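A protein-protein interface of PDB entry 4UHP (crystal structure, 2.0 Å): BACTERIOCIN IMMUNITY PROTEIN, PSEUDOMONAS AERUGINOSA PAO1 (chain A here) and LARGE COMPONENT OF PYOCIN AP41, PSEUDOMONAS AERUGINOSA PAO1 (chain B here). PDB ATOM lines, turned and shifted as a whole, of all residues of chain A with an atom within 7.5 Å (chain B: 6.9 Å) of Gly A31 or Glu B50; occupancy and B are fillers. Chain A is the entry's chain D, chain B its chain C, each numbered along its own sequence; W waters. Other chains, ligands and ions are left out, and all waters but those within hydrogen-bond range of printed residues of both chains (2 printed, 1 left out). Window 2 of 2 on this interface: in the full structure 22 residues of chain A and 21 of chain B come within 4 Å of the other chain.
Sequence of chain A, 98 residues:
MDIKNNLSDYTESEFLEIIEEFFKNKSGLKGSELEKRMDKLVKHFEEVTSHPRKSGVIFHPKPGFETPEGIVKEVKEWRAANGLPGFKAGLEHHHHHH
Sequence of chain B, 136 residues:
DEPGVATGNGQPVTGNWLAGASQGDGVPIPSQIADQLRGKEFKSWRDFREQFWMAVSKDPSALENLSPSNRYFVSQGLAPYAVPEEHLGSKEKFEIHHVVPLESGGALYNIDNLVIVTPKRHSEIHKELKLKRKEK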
ATOM      1  N   ASN A  25     -15.534  24.384 -29.075  1.00  0.00           N
ATOM      2  CA  ASN A  25     -16.056  23.190 -29.729  1.00  0.00           C
ATOM      3  C   ASN A  25     -16.059  23.336 -31.245  1.00  0.00           C
ATOM      4  O   ASN A  25     -17.107  23.544 -31.854  1.00  0.00           O
ATOM      5  CB  ASN A  25     -17.469  22.881 -29.231  1.00  0.00           C
ATOM      6  CG  ASN A  25     -17.897  21.463 -29.543  1.00  0.00           C
ATOM      7  OD1 ASN A  25     -17.258  20.768 -30.334  1.00  0.00           O
ATOM      8  ND2 ASN A  25     -18.986  21.024 -28.924  1.00  0.00           N
ATOM      9  N   GLY A  28     -17.895  20.248 -33.046  1.00  0.00           N
ATOM     10  CA  GLY A  28     -19.335  20.204 -32.858  1.00  0.00           C
ATOM     11  C   GLY A  28     -19.763  18.922 -32.169  1.00  0.00           C
ATOM     12  O   GLY A  28     -20.938  18.734 -31.846  1.00  0.00           O
ATOM     13  N   LEU A  29     -18.796  18.040 -31.943  1.00  0.00           N
ATOM     14  CA  LEU A  29     -19.054  16.754 -31.308  1.00  0.00           C
ATOM     15  C   LEU A  29     -19.466  16.927 -29.851  1.00  0.00           C
ATOM     16  O   LEU A  29     -19.101  17.908 -29.201  1.00  0.00           O
ATOM     17  CB  LEU A  29     -17.818  15.856 -31.399  1.00  0.00           C
ATOM     18  CG  LEU A  29     -17.299  15.558 -32.806  1.00  0.00           C
ATOM     19  CD1 LEU A  29     -16.049  14.690 -32.738  1.00  0.00           C
ATOM     20  CD2 LEU A  29     -18.377  14.890 -33.644  1.00  0.00           C
ATOM     21  N   LYS A  30     -20.230  15.968 -29.342  1.00  0.00           N
ATOM     22  CA  LYS A  30     -20.687  16.024 -27.960  1.00  0.00           C
ATOM     23  C   LYS A  30     -20.474  14.691 -27.251  1.00  0.00           C
ATOM     24  O   LYS A  30     -20.303  13.655 -27.893  1.00  0.00           O
ATOM     25  CB  LYS A  30     -22.165  16.423 -27.905  1.00  0.00           C
ATOM     26  CG  LYS A  30     -22.436  17.837 -28.403  1.00  0.00           C
ATOM     27  CD  LYS A  30     -23.919  18.169 -28.375  1.00  0.00           C
ATOM     28  CE  LYS A  30     -24.697  17.306 -29.352  1.00  0.00           C
ATOM     29  NZ  LYS A  30     -26.132  17.701 -29.417  1.00  0.00           N
ATOM     30  N   GLY A  31     -20.473  14.734 -25.922  1.00  0.00           N
ATOM     31  CA  GLY A  31     -20.398  13.536 -25.107  1.00  0.00           C
ATOM     32  C   GLY A  31     -19.153  12.695 -25.315  1.00  0.00           C
ATOM     33  O   GLY A  31     -18.031  13.204 -25.309  1.00  0.00           O
ATOM     34  N   SER A  32     -19.361  11.395 -25.500  1.00  0.00           N
ATOM     35  CA  SER A  32     -18.260  10.450 -25.621  1.00  0.00           C
ATOM     36  C   SER A  32     -17.461  10.646 -26.906  1.00  0.00           C
ATOM     37  O   SER A  32     -16.251  10.443 -26.919  1.00  0.00           O
ATOM     38  CB  SER A  32     -18.783   9.013 -25.544  1.00  0.00           C
ATOM     39  OG  SER A  32     -19.803   8.783 -26.501  1.00  0.00           O
ATOM     40  N   GLU A  33     -18.134  11.043 -27.983  1.00  0.00           N
ATOM     41  CA  GLU A  33     -17.456  11.245 -29.261  1.00  0.00           C
ATOM     42  C   GLU A  33     -16.523  12.446 -29.210  1.00  0.00           C
ATOM     43  O   GLU A  33     -15.443  12.430 -29.805  1.00  0.00           O
ATOM     44  CB  GLU A  33     -18.469  11.426 -30.391  1.00  0.00           C
ATOM     45  CG  GLU A  33     -19.163  10.144 -30.804  1.00  0.00           C
ATOM     46  CD  GLU A  33     -19.872  10.272 -32.134  1.00  0.00           C
ATOM     47  OE1 GLU A  33     -20.119  11.416 -32.574  1.00  0.00           O
ATOM     48  OE2 GLU A  33     -20.179   9.227 -32.742  1.00  0.00           O
ATOM     49  N   LEU A  34     -16.949  13.488 -28.506  1.00  0.00           N
ATOM     50  CA  LEU A  34     -16.120  14.670 -28.330  1.00  0.00           C
ATOM     51  C   LEU A  34     -14.890  14.314 -27.510  1.00  0.00           C
ATOM     52  O   LEU A  34     -13.776  14.726 -27.830  1.00  0.00           O
ATOM     53  CB  LEU A  34     -16.907  15.792 -27.653  1.00  0.00           C
ATOM     54  CG  LEU A  34     -16.117  17.057 -27.311  1.00  0.00           C
ATOM     55  CD1 LEU A  34     -15.504  17.667 -28.564  1.00  0.00           C
ATOM     56  CD2 LEU A  34     -17.002  18.067 -26.599  1.00  0.00           C
ATOM     57  N   GLU A  35     -15.102  13.528 -26.461  1.00  0.00           N
ATOM     58  CA  GLU A  35     -14.021  13.168 -25.554  1.00  0.00           C
ATOM     59  C   GLU A  35     -12.964  12.317 -26.247  1.00  0.00           C
ATOM     60  O   GLU A  35     -11.770  12.496 -26.016  1.00  0.00           O
ATOM     61  CB  GLU A  35     -14.565  12.431 -24.331  1.00  0.00           C
ATOM     62  CG  GLU A  35     -13.530  12.234 -23.241  1.00  0.00           C
ATOM     63  CD  GLU A  35     -14.151  12.031 -21.878  1.00  0.00           C
ATOM     64  OE1 GLU A  35     -15.360  11.721 -21.812  1.00  0.00           O
ATOM     65  OE2 GLU A  35     -13.432  12.192 -20.870  1.00  0.00           O
ATOM     66  N   LYS A  36     -13.401  11.392 -27.096  1.00  0.00           N
ATOM     67  CA  LYS A  36     -12.462  10.527 -27.801  1.00  0.00           C
ATOM     68  C   LYS A  36     -11.675  11.302 -28.858  1.00  0.00           C
ATOM     69  O   LYS A  36     -10.543  10.944 -29.180  1.00  0.00           O
ATOM     70  CB  LYS A  36     -13.191   9.342 -28.437  1.00  0.00           C
ATOM     71  CG  LYS A  36     -13.867   8.426 -27.427  1.00  0.00           C
ATOM     72  CD  LYS A  36     -13.590   6.961 -27.724  1.00  0.00           C
ATOM     73  CE  LYS A  36     -13.298   6.182 -26.449  1.00  0.00           C
ATOM     74  NZ  LYS A  36     -11.844   6.170 -26.123  1.00  0.00           N
ATOM     75  N   ARG A  37     -12.269  12.365 -29.392  1.00  0.00           N
ATOM     76  CA  ARG A  37     -11.538  13.240 -30.302  1.00  0.00           C
ATOM     77  C   ARG A  37     -10.491  14.043 -29.539  1.00  0.00           C
ATOM     78  O   ARG A  37      -9.349  14.167 -29.981  1.00  0.00           O
ATOM     79  CB  ARG A  37     -12.480  14.189 -31.048  1.00  0.00           C
ATOM     80  CG  ARG A  37     -11.736  15.322 -31.747  1.00  0.00           C
ATOM     81  CD  ARG A  37     -12.574  16.033 -32.794  1.00  0.00           C
ATOM     82  NE  ARG A  37     -11.794  17.078 -33.453  1.00  0.00           N
ATOM     83  CZ  ARG A  37     -10.992  16.870 -34.493  1.00  0.00           C
ATOM     84  NH1 ARG A  37     -10.870  15.653 -35.007  1.00  0.00           N
ATOM     85  NH2 ARG A  37     -10.314  17.878 -35.022  1.00  0.00           N
ATOM     86  N   PHE B  42     -30.261   9.372 -13.820  1.00  0.00           N
ATOM     87  CA  PHE B  42     -29.234   9.208 -14.837  1.00  0.00           C
ATOM     88  C   PHE B  42     -29.404   7.872 -15.548  1.00  0.00           C
ATOM     89  O   PHE B  42     -29.626   6.844 -14.911  1.00  0.00           O
ATOM     90  CB  PHE B  42     -27.844   9.329 -14.211  1.00  0.00           C
ATOM     91  CG  PHE B  42     -27.628  10.621 -13.474  1.00  0.00           C
ATOM     92  CD1 PHE B  42     -27.132  11.735 -14.132  1.00  0.00           C
ATOM     93  CD2 PHE B  42     -27.938  10.728 -12.129  1.00  0.00           C
ATOM     94  CE1 PHE B  42     -26.941  12.929 -13.458  1.00  0.00           C
ATOM     95  CE2 PHE B  42     -27.751  11.919 -11.451  1.00  0.00           C
ATOM     96  CZ  PHE B  42     -27.250  13.021 -12.117  1.00  0.00           C
ATOM     97  N   LYS B  43     -29.308   7.900 -16.873  1.00  0.00           N
ATOM     98  CA  LYS B  43     -29.592   6.726 -17.689  1.00  0.00           C
ATOM     99  C   LYS B  43     -28.442   5.726 -17.664  1.00  0.00           C
ATOM    100  O   LYS B  43     -28.643   4.530 -17.873  1.00  0.00           O
ATOM    101  CB  LYS B  43     -29.895   7.146 -19.128  1.00  0.00           C
ATOM    102  CG  LYS B  43     -30.703   8.430 -19.233  1.00  0.00           C
ATOM    103  CD  LYS B  43     -30.582   9.049 -20.616  1.00  0.00           C
ATOM    104  CE  LYS B  43     -30.529  10.565 -20.543  1.00  0.00           C
ATOM    105  NZ  LYS B  43     -29.131  11.054 -20.399  1.00  0.00           N
ATOM    106  N   TRP B  45     -23.886   5.376 -16.217  1.00  0.00           N
ATOM    107  CA  TRP B  45     -22.780   5.984 -15.488  1.00  0.00           C
ATOM    108  C   TRP B  45     -22.111   7.050 -16.346  1.00  0.00           C
ATOM    109  O   TRP B  45     -21.717   8.103 -15.844  1.00  0.00           O
ATOM    110  CB  TRP B  45     -21.756   4.932 -15.054  1.00  0.00           C
ATOM    111  CG  TRP B  45     -20.582   5.533 -14.340  1.00  0.00           C
ATOM    112  CD1 TRP B  45     -19.303   5.642 -14.809  1.00  0.00           C
ATOM    113  CD2 TRP B  45     -20.584   6.135 -13.042  1.00  0.00           C
ATOM    114  NE1 TRP B  45     -18.508   6.264 -13.877  1.00  0.00           N
ATOM    115  CE2 TRP B  45     -19.273   6.579 -12.780  1.00  0.00           C
ATOM    116  CE3 TRP B  45     -21.571   6.343 -12.069  1.00  0.00           C
ATOM    117  CZ2 TRP B  45     -18.916   7.211 -11.592  1.00  0.00           C
ATOM    118  CZ3 TRP B  45     -21.218   6.971 -10.888  1.00  0.00           C
ATOM    119  CH2 TRP B  45     -19.902   7.398 -10.659  1.00  0.00           C
ATOM    120  N   ARG B  46     -21.988   6.767 -17.640  1.00  0.00           N
ATOM    121  CA  ARG B  46     -21.452   7.728 -18.597  1.00  0.00           C
ATOM    122  C   ARG B  46     -22.272   9.011 -18.568  1.00  0.00           C
ATOM    123  O   ARG B  46     -21.727  10.109 -18.650  1.00  0.00           O
ATOM    124  CB  ARG B  46     -21.438   7.135 -20.009  1.00  0.00           C
ATOM    125  CG  ARG B  46     -21.017   8.118 -21.092  1.00  0.00           C
ATOM    126  CD  ARG B  46     -19.584   8.590 -20.892  1.00  0.00           C
ATOM    127  NE  ARG B  46     -19.318   9.841 -21.597  1.00  0.00           N
ATOM    128  CZ  ARG B  46     -18.126  10.425 -21.665  1.00  0.00           C
ATOM    129  NH1 ARG B  46     -17.076   9.867 -21.076  1.00  0.00           N
ATOM    130  NH2 ARG B  46     -17.980  11.566 -22.327  1.00  0.00           N
ATOM    131  N   ASP B  47     -23.587   8.860 -18.438  1.00  0.00           N
ATOM    132  CA  ASP B  47     -24.487  10.003 -18.338  1.00  0.00           C
ATOM    133  C   ASP B  47     -24.219  10.796 -17.063  1.00  0.00           C
ATOM    134  O   ASP B  47     -24.169  12.027 -17.085  1.00  0.00           O
ATOM    135  CB  ASP B  47     -25.944   9.542 -18.380  1.00  0.00           C
ATOM    136  CG  ASP B  47     -26.927  10.690 -18.227  1.00  0.00           C
ATOM    137  OD1 ASP B  47     -26.624  11.807 -18.693  1.00  0.00           O
ATOM    138  OD2 ASP B  47     -28.007  10.471 -17.641  1.00  0.00           O
ATOM    139  N   PHE B  48     -24.038  10.087 -15.953  1.00  0.00           N
ATOM    140  CA  PHE B  48     -23.755  10.737 -14.678  1.00  0.00           C
ATOM    141  C   PHE B  48     -22.416  11.466 -14.702  1.00  0.00           C
ATOM    142  O   PHE B  48     -22.294  12.576 -14.182  1.00  0.00           O
ATOM    143  CB  PHE B  48     -23.762   9.722 -13.534  1.00  0.00           C
ATOM    144  CG  PHE B  48     -23.389  10.313 -12.204  1.00  0.00           C
ATOM    145  CD1 PHE B  48     -24.340  10.952 -11.426  1.00  0.00           C
ATOM    146  CD2 PHE B  48     -22.088  10.242 -11.735  1.00  0.00           C
ATOM    147  CE1 PHE B  48     -24.000  11.506 -10.207  1.00  0.00           C
ATOM    148  CE2 PHE B  48     -21.742  10.795 -10.518  1.00  0.00           C
ATOM    149  CZ  PHE B  48     -22.700  11.426  -9.751  1.00  0.00           C
ATOM    150  N   ARG B  49     -21.414  10.824 -15.297  1.00  0.00           N
ATOM    151  CA  ARG B  49     -20.076  11.392 -15.392  1.00  0.00           C
ATOM    152  C   ARG B  49     -20.095  12.710 -16.155  1.00  0.00           C
ATOM    153  O   ARG B  49     -19.455  13.677 -15.751  1.00  0.00           O
ATOM    154  CB  ARG B  49     -19.122  10.402 -16.066  1.00  0.00           C
ATOM    155  CG  ARG B  49     -17.764  10.989 -16.416  1.00  0.00           C
ATOM    156  CD  ARG B  49     -16.837   9.959 -17.056  1.00  0.00           C
ATOM    157  NE  ARG B  49     -15.630  10.586 -17.588  1.00  0.00           N
ATOM    158  CZ  ARG B  49     -14.624   9.927 -18.156  1.00  0.00           C
ATOM    159  NH1 ARG B  49     -14.671   8.607 -18.270  1.00  0.00           N
ATOM    160  NH2 ARG B  49     -13.569  10.590 -18.610  1.00  0.00           N
ATOM    161  N   GLU B  50     -20.839  12.747 -17.255  1.00  0.00           N
ATOM    162  CA  GLU B  50     -20.964  13.967 -18.042  1.00  0.00           C
ATOM    163  C   GLU B  50     -21.630  15.069 -17.226  1.00  0.00           C
ATOM    164  O   GLU B  50     -21.181  16.215 -17.225  1.00  0.00           O
ATOM    165  CB  GLU B  50     -21.755  13.706 -19.324  1.00  0.00           C
ATOM    166  CG  GLU B  50     -21.033  12.819 -20.317  1.00  0.00           C
ATOM    167  CD  GLU B  50     -21.818  12.618 -21.593  1.00  0.00           C
ATOM    168  OE1 GLU B  50     -22.911  13.211 -21.716  1.00  0.00           O
ATOM    169  OE2 GLU B  50     -21.340  11.870 -22.472  1.00  0.00           O
ATOM    170  N   GLN B  51     -22.698  14.710 -16.524  1.00  0.00           N
ATOM    171  CA  GLN B  51     -23.451  15.673 -15.732  1.00  0.00           C
ATOM    172  C   GLN B  51     -22.639  16.168 -14.543  1.00  0.00           C
ATOM    173  O   GLN B  51     -22.792  17.310 -14.111  1.00  0.00           O
ATOM    174  CB  GLN B  51     -24.765  15.056 -15.248  1.00  0.00           C
ATOM    175  CG  GLN B  51     -25.734  14.701 -16.364  1.00  0.00           C
ATOM    176  CD  GLN B  51     -26.179  15.913 -17.157  1.00  0.00           C
ATOM    177  OE1 GLN B  51     -26.874  16.787 -16.638  1.00  0.00           O
ATOM    178  NE2 GLN B  51     -25.781  15.973 -18.422  1.00  0.00           N
ATOM    179  N   PHE B  52     -21.782  15.304 -14.013  1.00  0.00           N
ATOM    180  CA  PHE B  52     -20.966  15.661 -12.863  1.00  0.00           C
ATOM    181  C   PHE B  52     -20.006  16.804 -13.193  1.00  0.00           C
ATOM    182  O   PHE B  52     -19.965  17.812 -12.486  1.00  0.00           O
ATOM    183  CB  PHE B  52     -20.177  14.450 -12.363  1.00  0.00           C
ATOM    184  CG  PHE B  52     -19.190  14.784 -11.282  1.00  0.00           C
ATOM    185  CD1 PHE B  52     -19.589  14.850  -9.960  1.00  0.00           C
ATOM    186  CD2 PHE B  52     -17.864  15.045 -11.591  1.00  0.00           C
ATOM    187  CE1 PHE B  52     -18.685  15.164  -8.967  1.00  0.00           C
ATOM    188  CE2 PHE B  52     -16.958  15.360 -10.601  1.00  0.00           C
ATOM    189  CZ  PHE B  52     -17.367  15.420  -9.290  1.00  0.00           C
ATOM    190  N   TRP B  53     -19.232  16.641 -14.260  1.00  0.00           N
ATOM    191  CA  TRP B  53     -18.265  17.663 -14.646  1.00  0.00           C
ATOM    192  C   TRP B  53     -18.961  18.940 -15.101  1.00  0.00           C
ATOM    193  O   TRP B  53     -18.489  20.038 -14.814  1.00  0.00           O
ATOM    194  CB  TRP B  53     -17.328  17.140 -15.737  1.00  0.00           C
ATOM    195  CG  TRP B  53     -16.464  16.024 -15.255  1.00  0.00           C
ATOM    196  CD1 TRP B  53     -16.438  14.747 -15.729  1.00  0.00           C
ATOM    197  CD2 TRP B  53     -15.517  16.071 -14.179  1.00  0.00           C
ATOM    198  NE1 TRP B  53     -15.527  13.999 -15.024  1.00  0.00           N
ATOM    199  CE2 TRP B  53     -14.951  14.788 -14.066  1.00  0.00           C
ATOM    200  CE3 TRP B  53     -15.095  17.075 -13.302  1.00  0.00           C
ATOM    201  CZ2 TRP B  53     -13.979  14.482 -13.115  1.00  0.00           C
ATOM    202  CZ3 TRP B  53     -14.132  16.770 -12.357  1.00  0.00           C
ATOM    203  CH2 TRP B  53     -13.585  15.484 -12.271  1.00  0.00           C
ATOM    204  N   MET B  54     -20.087  18.800 -15.794  1.00  0.00           N
ATOM    205  CA  MET B  54     -20.881  19.965 -16.173  1.00  0.00           C
ATOM    206  C   MET B  54     -21.331  20.736 -14.936  1.00  0.00           C
ATOM    207  O   MET B  54     -21.439  21.959 -14.968  1.00  0.00           O
ATOM    208  CB  MET B  54     -22.094  19.556 -17.013  1.00  0.00           C
ATOM    209  CG  MET B  54     -21.751  19.263 -18.465  1.00  0.00           C
ATOM    210  SD  MET B  54     -23.193  18.938 -19.494  1.00  0.00           S
ATOM    211  CE  MET B  54     -24.054  20.505 -19.372  1.00  0.00           C
ATOM    212  N   ALA B  55     -21.581  20.020 -13.844  1.00  0.00           N
ATOM    213  CA  ALA B  55     -21.925  20.668 -12.584  1.00  0.00           C
ATOM    214  C   ALA B  55     -20.687  21.331 -11.988  1.00  0.00           C
ATOM    215  O   ALA B  55     -20.771  22.403 -11.393  1.00  0.00           O
ATOM    216  CB  ALA B  55     -22.525  19.670 -11.606  1.00  0.00           C
ATOM    217  N   VAL B  74     -14.663  20.814 -18.792  1.00  0.00           N
ATOM    218  CA  VAL B  74     -15.738  20.492 -17.853  1.00  0.00           C
ATOM    219  C   VAL B  74     -17.064  21.103 -18.310  1.00  0.00           C
ATOM    220  O   VAL B  74     -18.135  20.587 -17.986  1.00  0.00           O
ATOM    221  CB  VAL B  74     -15.419  20.967 -16.413  1.00  0.00           C
ATOM    222  CG1 VAL B  74     -14.266  20.160 -15.828  1.00  0.00           C
ATOM    223  CG2 VAL B  74     -15.105  22.457 -16.383  1.00  0.00           C
ATOM    224  N   GLN B  76     -18.084  21.015 -21.232  1.00  0.00           N
ATOM    225  CA  GLN B  76     -18.597  20.100 -22.246  1.00  0.00           C
ATOM    226  C   GLN B  76     -18.896  18.721 -21.662  1.00  0.00           C
ATOM    227  O   GLN B  76     -19.211  17.779 -22.392  1.00  0.00           O
ATOM    228  CB  GLN B  76     -17.602  19.972 -23.398  1.00  0.00           C
ATOM    229  CG  GLN B  76     -17.253  21.297 -24.048  1.00  0.00           C
ATOM    230  CD  GLN B  76     -18.471  22.006 -24.613  1.00  0.00           C
ATOM    231  OE1 GLN B  76     -19.161  21.479 -25.486  1.00  0.00           O
ATOM    232  NE2 GLN B  76     -18.745  23.204 -24.109  1.00  0.00           N
ATOM    233  N   GLY B  77     -18.785  18.607 -20.345  1.00  0.00           N
ATOM    234  CA  GLY B  77     -19.015  17.343 -19.667  1.00  0.00           C
ATOM    235  C   GLY B  77     -17.818  16.415 -19.736  1.00  0.00           C
ATOM    236  O   GLY B  77     -17.937  15.221 -19.464  1.00  0.00           O
ATOM    237  N   LEU B  78     -16.661  16.962 -20.098  1.00  0.00           N
ATOM    238  CA  LEU B  78     -15.445  16.165 -20.206  1.00  0.00           C
ATOM    239  C   LEU B  78     -14.618  16.266 -18.932  1.00  0.00           C
ATOM    240  O   LEU B  78     -14.539  17.329 -18.318  1.00  0.00           O
ATOM    241  CB  LEU B  78     -14.610  16.609 -21.411  1.00  0.00           C
ATOM    242  CG  LEU B  78     -15.319  16.668 -22.765  1.00  0.00           C
ATOM    243  CD1 LEU B  78     -14.319  16.911 -23.889  1.00  0.00           C
ATOM    244  CD2 LEU B  78     -16.120  15.403 -23.017  1.00  0.00           C
ATOM    245  N   ILE B  96     -13.564   9.895 -11.389  1.00  0.00           N
ATOM    246  CA  ILE B  96     -14.578   9.605 -10.385  1.00  0.00           C
ATOM    247  C   ILE B  96     -14.471   8.141  -9.990  1.00  0.00           C
ATOM    248  O   ILE B  96     -14.468   7.257 -10.850  1.00  0.00           O
ATOM    249  CB  ILE B  96     -15.998   9.888 -10.896  1.00  0.00           C
ATOM    250  CG1 ILE B  96     -16.091  11.299 -11.472  1.00  0.00           C
ATOM    251  CG2 ILE B  96     -17.011   9.698  -9.776  1.00  0.00           C
ATOM    252  CD1 ILE B  96     -17.428  11.600 -12.109  1.00  0.00           C
HETATM  253  O   HOH W   1     -16.157  12.826 -18.841  1.00  0.00           O
HETATM  254  O   HOH W   2     -20.434  17.290 -24.489  1.00  0.00           O
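O of Gly A31 lies close to NH2 of Arg B46. OE1 of Glu A35 lies within salt-bridge range of NH1 of Arg B46 (2.6 Å). NH2 of Arg B49 is in salt-bridge range of OE2 of Glu A35. The side-chain amide oxygen (OE1) of Gln B76 sits at hydrogen-bond distance from the side-chain amide nitrogen (ND2) of Asn A25 (3.5 Å). The guanidinium group (NH2) of Arg B46 sits close to the backbone NH (N) of Ser A32, at 3.5 Å.
The guanidinium group (NE) of Arg B46 is in salt-bridge range of the side-chain carboxylate (OE2) of Glu B50 (3.0 Å). The side-chain amide oxygen (OD1) of Asn A25 lies within hydrogen-bond range of the backbone NH (N) of Gly A28, at 2.8 Å. O of Leu A29 lies within hydrogen-bond range of ND2 of Asn A25 (3.1 Å).
Among the printed residues, merely in contact across the chains: Gly A31 with Glu B50 (3.3 Å), Gly A31 with Leu B78 (3.7 Å), Ser A32 with Glu B50 (3.6 Å), Leu A34 with Gln B76 (3.8 Å), Leu A34 with Leu B78 (3.9 Å) and Glu A35 with Leu B78 (3.6 Å).
Glu B50 touches just these residues of chain A: Gly A31 (3.3 Å) and Ser A32 (3.6 Å). Of the printed residues of chain A, Leu B78 touches Gly A31, Leu A34 and Glu A35. Of the printed residues of chain B, Leu A34 touches Gln B76 (3.8 Å) and Leu B78 (3.9 Å). Printed residues of chain B within 4 Å of Ser A32: Arg B46 (3.5 Å) and Glu B50 (3.6 Å). Printed residues of chain A within 4 Å of Gln B76: Asn A25 and Leu A34. The nearest residue of chain A that does not touch Glu B50 is Lys A30 (5.6 Å). The nearest printed residue of chain B that does not touch Ser A32 is Leu B78 (5.7 Å).
Hydrophobic or aromatic side chains of chain B within 4 Å of the printed part of chain A: Leu B78. Hydrophobic or aromatic side chains of chain A within 4 Å of the printed part of chain B: Leu A34. Along chain A the printed residues that touch a printed residue of chain B span positions 25 to 35. Among the printed residues, 11 pairs touch across the chains.
Water W2 lies within hydrogen-bond range of O of Gln B76 (2.5 Å) and N of Gly A31 (2.9 Å). Water W1 lies within hydrogen-bond range of NE of Arg B49 (2.6 Å), O of Gly B77 (3.0 Å) and OE1 of Glu A35 (3.3 Å).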
